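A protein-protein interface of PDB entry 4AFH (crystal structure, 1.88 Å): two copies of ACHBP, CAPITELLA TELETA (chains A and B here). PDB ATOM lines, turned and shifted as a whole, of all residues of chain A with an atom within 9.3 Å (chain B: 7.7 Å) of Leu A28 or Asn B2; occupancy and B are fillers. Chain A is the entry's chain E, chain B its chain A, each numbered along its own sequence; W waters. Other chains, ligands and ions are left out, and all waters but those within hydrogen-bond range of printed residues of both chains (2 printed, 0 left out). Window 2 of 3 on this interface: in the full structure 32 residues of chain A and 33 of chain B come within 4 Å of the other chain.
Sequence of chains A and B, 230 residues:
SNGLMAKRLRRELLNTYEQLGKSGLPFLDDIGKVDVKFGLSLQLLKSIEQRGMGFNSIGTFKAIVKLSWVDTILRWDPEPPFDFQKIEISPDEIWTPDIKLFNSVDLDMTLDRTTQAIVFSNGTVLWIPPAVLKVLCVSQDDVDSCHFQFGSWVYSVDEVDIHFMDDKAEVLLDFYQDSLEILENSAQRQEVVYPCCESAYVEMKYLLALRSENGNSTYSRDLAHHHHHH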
ATOM      1  N   GLU A  12      10.005  19.707  10.477  1.00  0.00           N
ATOM      2  CA  GLU A  12       9.076  19.241  11.496  1.00  0.00           C
ATOM      3  C   GLU A  12       8.168  20.382  11.931  1.00  0.00           C
ATOM      4  O   GLU A  12       6.949  20.223  11.975  1.00  0.00           O
ATOM      5  CB  GLU A  12       9.808  18.632  12.696  1.00  0.00           C
ATOM      6  CG  GLU A  12      10.390  17.248  12.438  1.00  0.00           C
ATOM      7  CD  GLU A  12      10.728  16.497  13.721  1.00  0.00           C
ATOM      8  OE1 GLU A  12      10.259  16.911  14.804  1.00  0.00           O
ATOM      9  OE2 GLU A  12      11.465  15.488  13.646  1.00  0.00           O
ATOM     10  N   LEU A  13       8.753  21.547  12.208  1.00  0.00           N
ATOM     11  CA  LEU A  13       7.967  22.674  12.692  1.00  0.00           C
ATOM     12  C   LEU A  13       6.954  23.145  11.651  1.00  0.00           C
ATOM     13  O   LEU A  13       5.804  23.444  11.984  1.00  0.00           O
ATOM     14  CB  LEU A  13       8.874  23.832  13.096  1.00  0.00           C
ATOM     15  CG  LEU A  13       9.666  23.607  14.375  1.00  0.00           C
ATOM     16  CD1 LEU A  13      10.660  24.725  14.552  1.00  0.00           C
ATOM     17  CD2 LEU A  13       8.729  23.508  15.589  1.00  0.00           C
ATOM     18  N   ASN A  15       5.680  21.433   9.197  1.00  0.00           N
ATOM     19  CA  ASN A  15       4.779  20.405   8.688  1.00  0.00           C
ATOM     20  C   ASN A  15       3.310  20.746   8.948  1.00  0.00           C
ATOM     21  O   ASN A  15       2.443  20.523   8.102  1.00  0.00           O
ATOM     22  CB  ASN A  15       5.117  19.041   9.260  1.00  0.00           C
ATOM     23  CG  ASN A  15       4.276  17.950   8.648  1.00  0.00           C
ATOM     24  OD1 ASN A  15       4.309  17.737   7.433  1.00  0.00           O
ATOM     25  ND2 ASN A  15       3.502  17.263   9.477  1.00  0.00           N
ATOM     26  N   THR A  16       3.045  21.315  10.121  1.00  0.00           N
ATOM     27  CA  THR A  16       1.707  21.775  10.453  1.00  0.00           C
ATOM     28  C   THR A  16       1.154  22.790   9.457  1.00  0.00           C
ATOM     29  O   THR A  16       0.013  22.679   9.010  1.00  0.00           O
ATOM     30  CB  THR A  16       1.687  22.392  11.859  1.00  0.00           C
ATOM     31  OG1 THR A  16       2.053  21.380  12.809  1.00  0.00           O
ATOM     32  CG2 THR A  16       0.306  22.930  12.181  1.00  0.00           C
ATOM     33  N   TYR A  17       1.959  23.791   9.113  1.00  0.00           N
ATOM     34  CA  TYR A  17       1.520  24.834   8.207  1.00  0.00           C
ATOM     35  C   TYR A  17       1.354  24.304   6.769  1.00  0.00           C
ATOM     36  O   TYR A  17       0.460  24.730   6.027  1.00  0.00           O
ATOM     37  CB  TYR A  17       2.500  26.001   8.247  1.00  0.00           C
ATOM     38  CG  TYR A  17       2.216  26.978   9.380  1.00  0.00           C
ATOM     39  CD1 TYR A  17       0.946  27.512   9.557  1.00  0.00           C
ATOM     40  CD2 TYR A  17       3.212  27.340  10.284  1.00  0.00           C
ATOM     41  CE1 TYR A  17       0.676  28.411  10.591  1.00  0.00           C
ATOM     42  CE2 TYR A  17       2.951  28.239  11.333  1.00  0.00           C
ATOM     43  CZ  TYR A  17       1.683  28.763  11.477  1.00  0.00           C
ATOM     44  OH  TYR A  17       1.415  29.649  12.488  1.00  0.00           O
ATOM     45  N   LEU A  20      -2.001  22.099   7.095  1.00  0.00           N
ATOM     46  CA  LEU A  20      -3.236  22.777   7.501  1.00  0.00           C
ATOM     47  C   LEU A  20      -3.404  24.166   6.899  1.00  0.00           C
ATOM     48  O   LEU A  20      -4.500  24.724   6.913  1.00  0.00           O
ATOM     49  CB  LEU A  20      -3.337  22.860   9.029  1.00  0.00           C
ATOM     50  CG  LEU A  20      -3.293  21.510   9.752  1.00  0.00           C
ATOM     51  CD1 LEU A  20      -2.998  21.712  11.234  1.00  0.00           C
ATOM     52  CD2 LEU A  20      -4.583  20.724   9.550  1.00  0.00           C
ATOM     53  N   GLY A  21      -2.318  24.717   6.369  1.00  0.00           N
ATOM     54  CA  GLY A  21      -2.356  26.040   5.787  1.00  0.00           C
ATOM     55  C   GLY A  21      -1.904  27.083   6.791  1.00  0.00           C
ATOM     56  O   GLY A  21      -1.850  26.817   7.997  1.00  0.00           O
ATOM     57  N   GLY A  24      -5.314  31.564   9.886  1.00  0.00           N
ATOM     58  CA  GLY A  24      -5.783  31.343  11.244  1.00  0.00           C
ATOM     59  C   GLY A  24      -4.738  31.708  12.283  1.00  0.00           C
ATOM     60  O   GLY A  24      -3.526  31.609  12.039  1.00  0.00           O
ATOM     61  N   LEU A  25      -5.222  32.130  13.447  1.00  0.00           N
ATOM     62  CA  LEU A  25      -4.357  32.589  14.520  1.00  0.00           C
ATOM     63  C   LEU A  25      -3.423  31.450  14.936  1.00  0.00           C
ATOM     64  O   LEU A  25      -3.822  30.300  14.936  1.00  0.00           O
ATOM     65  CB  LEU A  25      -5.194  33.106  15.704  1.00  0.00           C
ATOM     66  CG  LEU A  25      -6.035  34.346  15.380  1.00  0.00           C
ATOM     67  CD1 LEU A  25      -6.991  34.708  16.530  1.00  0.00           C
ATOM     68  CD2 LEU A  25      -5.139  35.531  15.031  1.00  0.00           C
ATOM     69  N   PRO A  26      -2.160  31.777  15.241  1.00  0.00           N
ATOM     70  CA  PRO A  26      -1.117  30.771  15.479  1.00  0.00           C
ATOM     71  C   PRO A  26      -1.216  30.091  16.852  1.00  0.00           C
ATOM     72  O   PRO A  26      -0.353  30.246  17.728  1.00  0.00           O
ATOM     73  CB  PRO A  26       0.177  31.579  15.337  1.00  0.00           C
ATOM     74  CG  PRO A  26      -0.201  32.947  15.772  1.00  0.00           C
ATOM     75  CD  PRO A  26      -1.616  33.149  15.254  1.00  0.00           C
ATOM     76  N   PHE A  27      -2.292  29.325  17.018  1.00  0.00           N
ATOM     77  CA  PHE A  27      -2.485  28.499  18.198  1.00  0.00           C
ATOM     78  C   PHE A  27      -2.844  27.080  17.780  1.00  0.00           C
ATOM     79  O   PHE A  27      -3.580  26.873  16.816  1.00  0.00           O
ATOM     80  CB  PHE A  27      -3.611  29.066  19.067  1.00  0.00           C
ATOM     81  CG  PHE A  27      -3.339  30.444  19.590  1.00  0.00           C
ATOM     82  CD1 PHE A  27      -2.602  30.622  20.757  1.00  0.00           C
ATOM     83  CD2 PHE A  27      -3.823  31.564  18.926  1.00  0.00           C
ATOM     84  CE1 PHE A  27      -2.347  31.887  21.253  1.00  0.00           C
ATOM     85  CE2 PHE A  27      -3.573  32.846  19.420  1.00  0.00           C
ATOM     86  CZ  PHE A  27      -2.833  33.006  20.585  1.00  0.00           C
ATOM     87  N   LEU A  28      -2.326  26.102  18.504  1.00  0.00           N
ATOM     88  CA  LEU A  28      -2.689  24.723  18.236  1.00  0.00           C
ATOM     89  C   LEU A  28      -3.670  24.268  19.306  1.00  0.00           C
ATOM     90  O   LEU A  28      -4.628  23.546  19.027  1.00  0.00           O
ATOM     91  CB  LEU A  28      -1.439  23.850  18.219  1.00  0.00           C
ATOM     92  CG  LEU A  28      -1.449  22.682  17.236  1.00  0.00           C
ATOM     93  CD1 LEU A  28      -1.833  23.137  15.824  1.00  0.00           C
ATOM     94  CD2 LEU A  28      -0.085  22.008  17.250  1.00  0.00           C
ATOM     95  N   ASP A  29      -3.437  24.718  20.535  1.00  0.00           N
ATOM     96  CA  ASP A  29      -4.360  24.435  21.622  1.00  0.00           C
ATOM     97  C   ASP A  29      -5.428  25.523  21.648  1.00  0.00           C
ATOM     98  O   ASP A  29      -5.900  25.965  20.598  1.00  0.00           O
ATOM     99  CB  ASP A  29      -3.620  24.359  22.961  1.00  0.00           C
ATOM    100  CG  ASP A  29      -2.484  23.339  22.952  1.00  0.00           C
ATOM    101  OD1 ASP A  29      -2.700  22.191  22.497  1.00  0.00           O
ATOM    102  OD2 ASP A  29      -1.371  23.690  23.402  1.00  0.00           O
ATOM    103  N   ASP A  30      -5.800  25.965  22.841  1.00  0.00           N
ATOM    104  CA  ASP A  30      -6.831  26.985  22.979  1.00  0.00           C
ATOM    105  C   ASP A  30      -6.446  28.265  22.244  1.00  0.00           C
ATOM    106  O   ASP A  30      -5.295  28.697  22.295  1.00  0.00           O
ATOM    107  CB  ASP A  30      -7.085  27.285  24.453  1.00  0.00           C
ATOM    108  CG  ASP A  30      -7.787  26.147  25.161  1.00  0.00           C
ATOM    109  OD1 ASP A  30      -8.764  25.603  24.596  1.00  0.00           O
ATOM    110  OD2 ASP A  30      -7.357  25.799  26.280  1.00  0.00           O
ATOM    111  N   ILE A  31      -7.405  28.857  21.550  1.00  0.00           N
ATOM    112  CA  ILE A  31      -7.115  30.054  20.767  1.00  0.00           C
ATOM    113  C   ILE A  31      -7.133  31.259  21.684  1.00  0.00           C
ATOM    114  O   ILE A  31      -8.165  31.592  22.271  1.00  0.00           O
ATOM    115  CB  ILE A  31      -8.114  30.256  19.631  1.00  0.00           C
ATOM    116  CG1 ILE A  31      -8.025  29.082  18.647  1.00  0.00           C
ATOM    117  CG2 ILE A  31      -7.839  31.569  18.917  1.00  0.00           C
ATOM    118  CD1 ILE A  31      -9.008  29.156  17.507  1.00  0.00           C
ATOM    119  N   GLY A  32      -5.981  31.898  21.826  1.00  0.00           N
ATOM    120  CA  GLY A  32      -5.886  33.091  22.645  1.00  0.00           C
ATOM    121  C   GLY A  32      -5.780  34.357  21.809  1.00  0.00           C
ATOM    122  O   GLY A  32      -6.376  34.484  20.734  1.00  0.00           O
ATOM    123  N   VAL A  70       4.237  35.827  19.249  1.00  0.00           N
ATOM    124  CA  VAL A  70       4.434  34.426  19.609  1.00  0.00           C
ATOM    125  C   VAL A  70       3.597  33.524  18.704  1.00  0.00           C
ATOM    126  O   VAL A  70       2.392  33.746  18.522  1.00  0.00           O
ATOM    127  CB  VAL A  70       4.119  34.171  21.104  1.00  0.00           C
ATOM    128  CG1 VAL A  70       4.305  32.689  21.463  1.00  0.00           C
ATOM    129  CG2 VAL A  70       5.030  35.022  21.966  1.00  0.00           C
ATOM    130  N   ASP A  71       4.261  32.537  18.105  1.00  0.00           N
ATOM    131  CA  ASP A  71       3.590  31.446  17.400  1.00  0.00           C
ATOM    132  C   ASP A  71       3.833  30.129  18.144  1.00  0.00           C
ATOM    133  O   ASP A  71       4.915  29.545  18.050  1.00  0.00           O
ATOM    134  CB  ASP A  71       4.089  31.361  15.938  1.00  0.00           C
ATOM    135  CG  ASP A  71       3.285  30.371  15.100  1.00  0.00           C
ATOM    136  OD1 ASP A  71       2.660  29.469  15.695  1.00  0.00           O
ATOM    137  OD2 ASP A  71       3.276  30.484  13.851  1.00  0.00           O
ATOM    138  N   THR A  72       2.819  29.650  18.862  1.00  0.00           N
ATOM    139  CA  THR A  72       2.969  28.448  19.690  1.00  0.00           C
ATOM    140  C   THR A  72       3.111  27.179  18.857  1.00  0.00           C
ATOM    141  O   THR A  72       3.525  26.143  19.366  1.00  0.00           O
ATOM    142  CB  THR A  72       1.788  28.266  20.666  1.00  0.00           C
ATOM    143  OG1 THR A  72       0.582  28.035  19.926  1.00  0.00           O
ATOM    144  CG2 THR A  72       1.618  29.503  21.554  1.00  0.00           C
ATOM    145  N   ILE A  73       2.758  27.257  17.574  1.00  0.00           N
ATOM    146  CA  ILE A  73       2.942  26.133  16.668  1.00  0.00           C
ATOM    147  C   ILE A  73       4.442  25.915  16.384  1.00  0.00           C
ATOM    148  O   ILE A  73       4.865  24.806  16.076  1.00  0.00           O
ATOM    149  CB  ILE A  73       2.135  26.325  15.333  1.00  0.00           C
ATOM    150  CG1 ILE A  73       0.625  26.366  15.604  1.00  0.00           C
ATOM    151  CG2 ILE A  73       2.446  25.218  14.309  1.00  0.00           C
ATOM    152  CD1 ILE A  73      -0.186  26.912  14.416  1.00  0.00           C
ATOM    153  N   LEU A  74       5.248  26.972  16.510  1.00  0.00           N
ATOM    154  CA  LEU A  74       6.661  26.879  16.138  1.00  0.00           C
ATOM    155  C   LEU A  74       7.595  26.741  17.340  1.00  0.00           C
ATOM    156  O   LEU A  74       8.690  27.286  17.345  1.00  0.00           O
ATOM    157  CB  LEU A  74       7.069  28.083  15.291  1.00  0.00           C
ATOM    158  CG  LEU A  74       6.226  28.359  14.040  1.00  0.00           C
ATOM    159  CD1 LEU A  74       6.557  29.736  13.456  1.00  0.00           C
ATOM    160  CD2 LEU A  74       6.414  27.253  12.995  1.00  0.00           C
ATOM    161  N   ARG A  75       7.153  26.019  18.364  1.00  0.00           N
ATOM    162  CA  ARG A  75       7.951  25.827  19.573  1.00  0.00           C
ATOM    163  C   ARG A  75       8.715  24.520  19.468  1.00  0.00           C
ATOM    164  O   ARG A  75       8.212  23.568  18.873  1.00  0.00           O
ATOM    165  CB  ARG A  75       7.032  25.680  20.794  1.00  0.00           C
ATOM    166  CG  ARG A  75       6.248  26.897  21.246  1.00  0.00           C
ATOM    167  CD  ARG A  75       5.165  26.418  22.219  1.00  0.00           C
ATOM    168  NE  ARG A  75       4.651  27.478  23.080  1.00  0.00           N
ATOM    169  CZ  ARG A  75       3.875  27.265  24.139  1.00  0.00           C
ATOM    170  NH1 ARG A  75       3.521  26.026  24.470  1.00  0.00           N
ATOM    171  NH2 ARG A  75       3.456  28.290  24.867  1.00  0.00           N
ATOM    172  N   SER B   1     -12.617  26.726  20.644  1.00  0.00           N
ATOM    173  CA  SER B   1     -12.106  25.361  20.561  1.00  0.00           C
ATOM    174  C   SER B   1     -10.612  25.390  20.253  1.00  0.00           C
ATOM    175  O   SER B   1      -9.956  26.413  20.442  1.00  0.00           O
ATOM    176  CB  SER B   1     -12.873  24.567  19.494  1.00  0.00           C
ATOM    177  OG  SER B   1     -12.430  23.220  19.404  1.00  0.00           O
ATOM    178  N   ASN B   2     -10.077  24.266  19.789  1.00  0.00           N
ATOM    179  CA  ASN B   2      -8.668  24.185  19.425  1.00  0.00           C
ATOM    180  C   ASN B   2      -8.367  25.010  18.178  1.00  0.00           C
ATOM    181  O   ASN B   2      -9.207  25.142  17.291  1.00  0.00           O
ATOM    182  CB  ASN B   2      -8.258  22.725  19.195  1.00  0.00           C
ATOM    183  CG  ASN B   2      -7.646  22.084  20.430  1.00  0.00           C
ATOM    184  OD1 ASN B   2      -6.508  21.613  20.400  1.00  0.00           O
ATOM    185  ND2 ASN B   2      -8.399  22.065  21.526  1.00  0.00           N
ATOM    186  N   GLY B   3      -7.162  25.564  18.114  1.00  0.00           N
ATOM    187  CA  GLY B   3      -6.716  26.248  16.917  1.00  0.00           C
ATOM    188  C   GLY B   3      -6.461  25.231  15.820  1.00  0.00           C
ATOM    189  O   GLY B   3      -6.461  25.569  14.628  1.00  0.00           O
ATOM    190  N   LEU B   4      -6.234  23.990  16.242  1.00  0.00           N
ATOM    191  CA  LEU B   4      -6.091  22.854  15.335  1.00  0.00           C
ATOM    192  C   LEU B   4      -7.400  22.600  14.603  1.00  0.00           C
ATOM    193  O   LEU B   4      -7.420  22.488  13.380  1.00  0.00           O
ATOM    194  CB  LEU B   4      -5.675  21.598  16.109  1.00  0.00           C
ATOM    195  CG  LEU B   4      -5.401  20.310  15.318  1.00  0.00           C
ATOM    196  CD1 LEU B   4      -4.159  20.463  14.444  1.00  0.00           C
ATOM    197  CD2 LEU B   4      -5.274  19.092  16.247  1.00  0.00           C
ATOM    198  N   MET B   5      -8.488  22.510  15.362  1.00  0.00           N
ATOM    199  CA  MET B   5      -9.809  22.260  14.808  1.00  0.00           C
ATOM    200  C   MET B   5     -10.279  23.383  13.891  1.00  0.00           C
ATOM    201  O   MET B   5     -11.042  23.145  12.959  1.00  0.00           O
ATOM    202  CB  MET B   5     -10.837  22.030  15.924  1.00  0.00           C
ATOM    203  CG  MET B   5     -10.680  20.710  16.676  1.00  0.00           C
ATOM    204  SD  MET B   5     -10.698  19.248  15.611  1.00  0.00           S
ATOM    205  CE  MET B   5      -8.946  18.878  15.531  1.00  0.00           C
ATOM    206  N   ALA B   6      -9.826  24.603  14.159  1.00  0.00           N
ATOM    207  CA  ALA B   6     -10.171  25.725  13.303  1.00  0.00           C
ATOM    208  C   ALA B   6      -9.485  25.559  11.946  1.00  0.00           C
ATOM    209  O   ALA B   6     -10.098  25.764  10.898  1.00  0.00           O
ATOM    210  CB  ALA B   6      -9.777  27.067  13.967  1.00  0.00           C
ATOM    211  N   LYS B   7      -8.213  25.178  11.959  1.00  0.00           N
ATOM    212  CA  LYS B   7      -7.519  24.935  10.699  1.00  0.00           C
ATOM    213  C   LYS B   7      -8.106  23.723   9.964  1.00  0.00           C
ATOM    214  O   LYS B   7      -8.203  23.727   8.735  1.00  0.00           O
ATOM    215  CB  LYS B   7      -6.013  24.754  10.911  1.00  0.00           C
ATOM    216  CG  LYS B   7      -5.284  26.021  11.333  1.00  0.00           C
ATOM    217  CD  LYS B   7      -3.819  25.735  11.661  1.00  0.00           C
ATOM    218  CE  LYS B   7      -3.066  27.011  12.055  1.00  0.00           C
ATOM    219  NZ  LYS B   7      -2.931  27.946  10.910  1.00  0.00           N
ATOM    220  N   ARG B   8      -8.506  22.692  10.709  1.00  0.00           N
ATOM    221  CA  ARG B   8      -9.092  21.523  10.065  1.00  0.00           C
ATOM    222  C   ARG B   8     -10.429  21.885   9.450  1.00  0.00           C
ATOM    223  O   ARG B   8     -10.745  21.446   8.346  1.00  0.00           O
ATOM    224  CB  ARG B   8      -9.244  20.351  11.029  1.00  0.00           C
ATOM    225  CG  ARG B   8      -7.928  19.719  11.452  1.00  0.00           C
ATOM    226  CD  ARG B   8      -8.108  18.219  11.685  1.00  0.00           C
ATOM    227  NE  ARG B   8      -7.306  17.698  12.792  1.00  0.00           N
ATOM    228  CZ  ARG B   8      -6.161  17.032  12.653  1.00  0.00           C
ATOM    229  NH1 ARG B   8      -5.660  16.802  11.442  1.00  0.00           N
ATOM    230  NH2 ARG B   8      -5.515  16.594  13.728  1.00  0.00           N
ATOM    231  N   PRO B  81     -16.922  19.599  17.157  1.00  0.00           N
ATOM    232  CA  PRO B  81     -15.653  20.263  17.463  1.00  0.00           C
ATOM    233  C   PRO B  81     -15.393  21.483  16.575  1.00  0.00           C
ATOM    234  O   PRO B  81     -14.277  21.999  16.555  1.00  0.00           O
ATOM    235  CB  PRO B  81     -14.636  19.178  17.133  1.00  0.00           C
ATOM    236  CG  PRO B  81     -15.241  18.509  15.927  1.00  0.00           C
ATOM    237  CD  PRO B  81     -16.750  18.561  16.124  1.00  0.00           C
ATOM    238  N   ASP B  83     -17.054  24.478  16.841  1.00  0.00           N
ATOM    239  CA  ASP B  83     -17.813  25.548  17.484  1.00  0.00           C
ATOM    240  C   ASP B  83     -17.164  26.914  17.241  1.00  0.00           C
ATOM    241  O   ASP B  83     -16.701  27.578  18.172  1.00  0.00           O
ATOM    242  CB  ASP B  83     -18.019  25.271  18.983  1.00  0.00           C
ATOM    243  CG  ASP B  83     -16.755  24.789  19.676  1.00  0.00           C
ATOM    244  OD1 ASP B  83     -16.027  23.947  19.100  1.00  0.00           O
ATOM    245  OD2 ASP B  83     -16.494  25.255  20.806  1.00  0.00           O
ATOM    246  N   PHE B  84     -17.131  27.300  15.967  1.00  0.00           N
ATOM    247  CA  PHE B  84     -16.642  28.601  15.533  1.00  0.00           C
ATOM    248  C   PHE B  84     -17.783  29.357  14.860  1.00  0.00           C
ATOM    249  O   PHE B  84     -18.605  28.771  14.150  1.00  0.00           O
ATOM    250  CB  PHE B  84     -15.456  28.430  14.573  1.00  0.00           C
ATOM    251  CG  PHE B  84     -14.363  27.549  15.124  1.00  0.00           C
ATOM    252  CD1 PHE B  84     -13.410  28.062  15.988  1.00  0.00           C
ATOM    253  CD2 PHE B  84     -14.312  26.197  14.813  1.00  0.00           C
ATOM    254  CE1 PHE B  84     -12.415  27.246  16.522  1.00  0.00           C
ATOM    255  CE2 PHE B  84     -13.315  25.376  15.343  1.00  0.00           C
ATOM    256  CZ  PHE B  84     -12.367  25.905  16.197  1.00  0.00           C
HETATM  257  O   HOH W   1      -5.973  28.503  13.924  1.00  0.00           O
HETATM  258  O   HOH W   2      -1.561  29.975  12.395  1.00  0.00           O
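The side-chain carboxylate (OD2) of Asp A71 sits at hydrogen-bond distance from the side-chain hydroxyl (OH) of Tyr A17 (2.5 Å).
The side-chain carboxylate of Asp A71 sits at hydrogen-bond distance from the backbone NH of Ile A73 (2.9 Å).
Leu A28 touches just these residues of chain B: Asn B2, Gly B3 and Leu B4.
Of chain A, only Leu A28 and Asp A29 come within 4 Å of Asn B2.
Of chain A, only Phe A27, Leu A28, Asp A29 and Ile A31 come within 4 Å of Gly B3.
Leu B4 touches three residues of chain A.
Of the printed residues of chain B, Ile A31 touches Ser B1 (3.7 Å) and Gly B3 (3.6 Å).
Printed residues of chain B within 4 Å of Phe A27: Gly B3 (3.2 Å) and Leu B4 (3.96 Å).
Of the printed residues of chain B, Ile A73 touches Lys B7 (3.7 Å).
Of the printed residues of chain B, Leu A20 touches Leu B4 (3.6 Å), Lys B7 (3.8 Å) and Arg B8 (3.98 Å).
The nearest residue of chain B that does not touch Leu A28 is Lys B7 (5.3 Å).
The nearest residue of chain A that does not touch Asn B2 is Ile A31 (4.02 Å).
The nearest printed residue of chain B that does not touch Phe A27 is Lys B7 (4.8 Å).
Of the 11 printed residues of chain B, 6 touch a printed residue of chain A.
Of the 22 printed residues of chain A, 9 touch a printed residue of chain B.
Printed residues of chain A that touch a printed residue of chain B: Tyr A17, Leu A20, Gly A21, Gly A24, Phe A27, Leu A28, Asp A29, Ile A31 and Ile A73.
No position is printed for both chains.
Of the 16 pairs that touch across the chains among the printed residues, none has its exchanged pair printed and touching as well.
Water W2 lies within hydrogen-bond range of O of Gly A24, NZ of Lys B7, OH of Tyr A17 and O of Leu A25.
Water W1 bridges the backbone carbonyl oxygen (O) of Leu A25 (3.0 Å) and the backbone carbonyl oxygen (O) of Gly B3 (3.1 Å).
Among the printed residues, pairs that only touch across the chains: Tyr A17 with Lys B7 (3.7 Å), Leu A20 with Leu B4 (3.6 Å), Leu A20 with Lys B7 (3.8 Å), Leu A20 with Arg B8 (3.98 Å), Gly A24 with Lys B7 (3.9 Å), Phe A27 with Gly B3 (3.2 Å), Phe A27 with Leu B4 (3.96 Å), Asp A29 with Asn B2 (3.5 Å), Ile A31 with Ser B1 (3.7 Å), Ile A31 with Gly B3 (3.6 Å) and Ile A73 with Lys B7 (3.7 Å).
The side-chain amide oxygen (OD1) of Asn B2 lies close to the backbone carbonyl oxygen (O) of Leu A28 (3.0 Å).
O of Leu A28 is in hydrogen-bond range of N of Gly B3 (3.4 Å).
The backbone NH (N) of Gly B3 lies within hydrogen-bond range of the backbone carbonyl oxygen (O) of Asp A29 (2.8 Å).
N of Leu B4 lies within hydrogen-bond range of O of Leu A28 (3.2 Å).
The side-chain amino group (NZ) of Lys B7 is in hydrogen-bond range of the backbone carbonyl oxygen (O) of Gly A21, at 3.3 Å.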
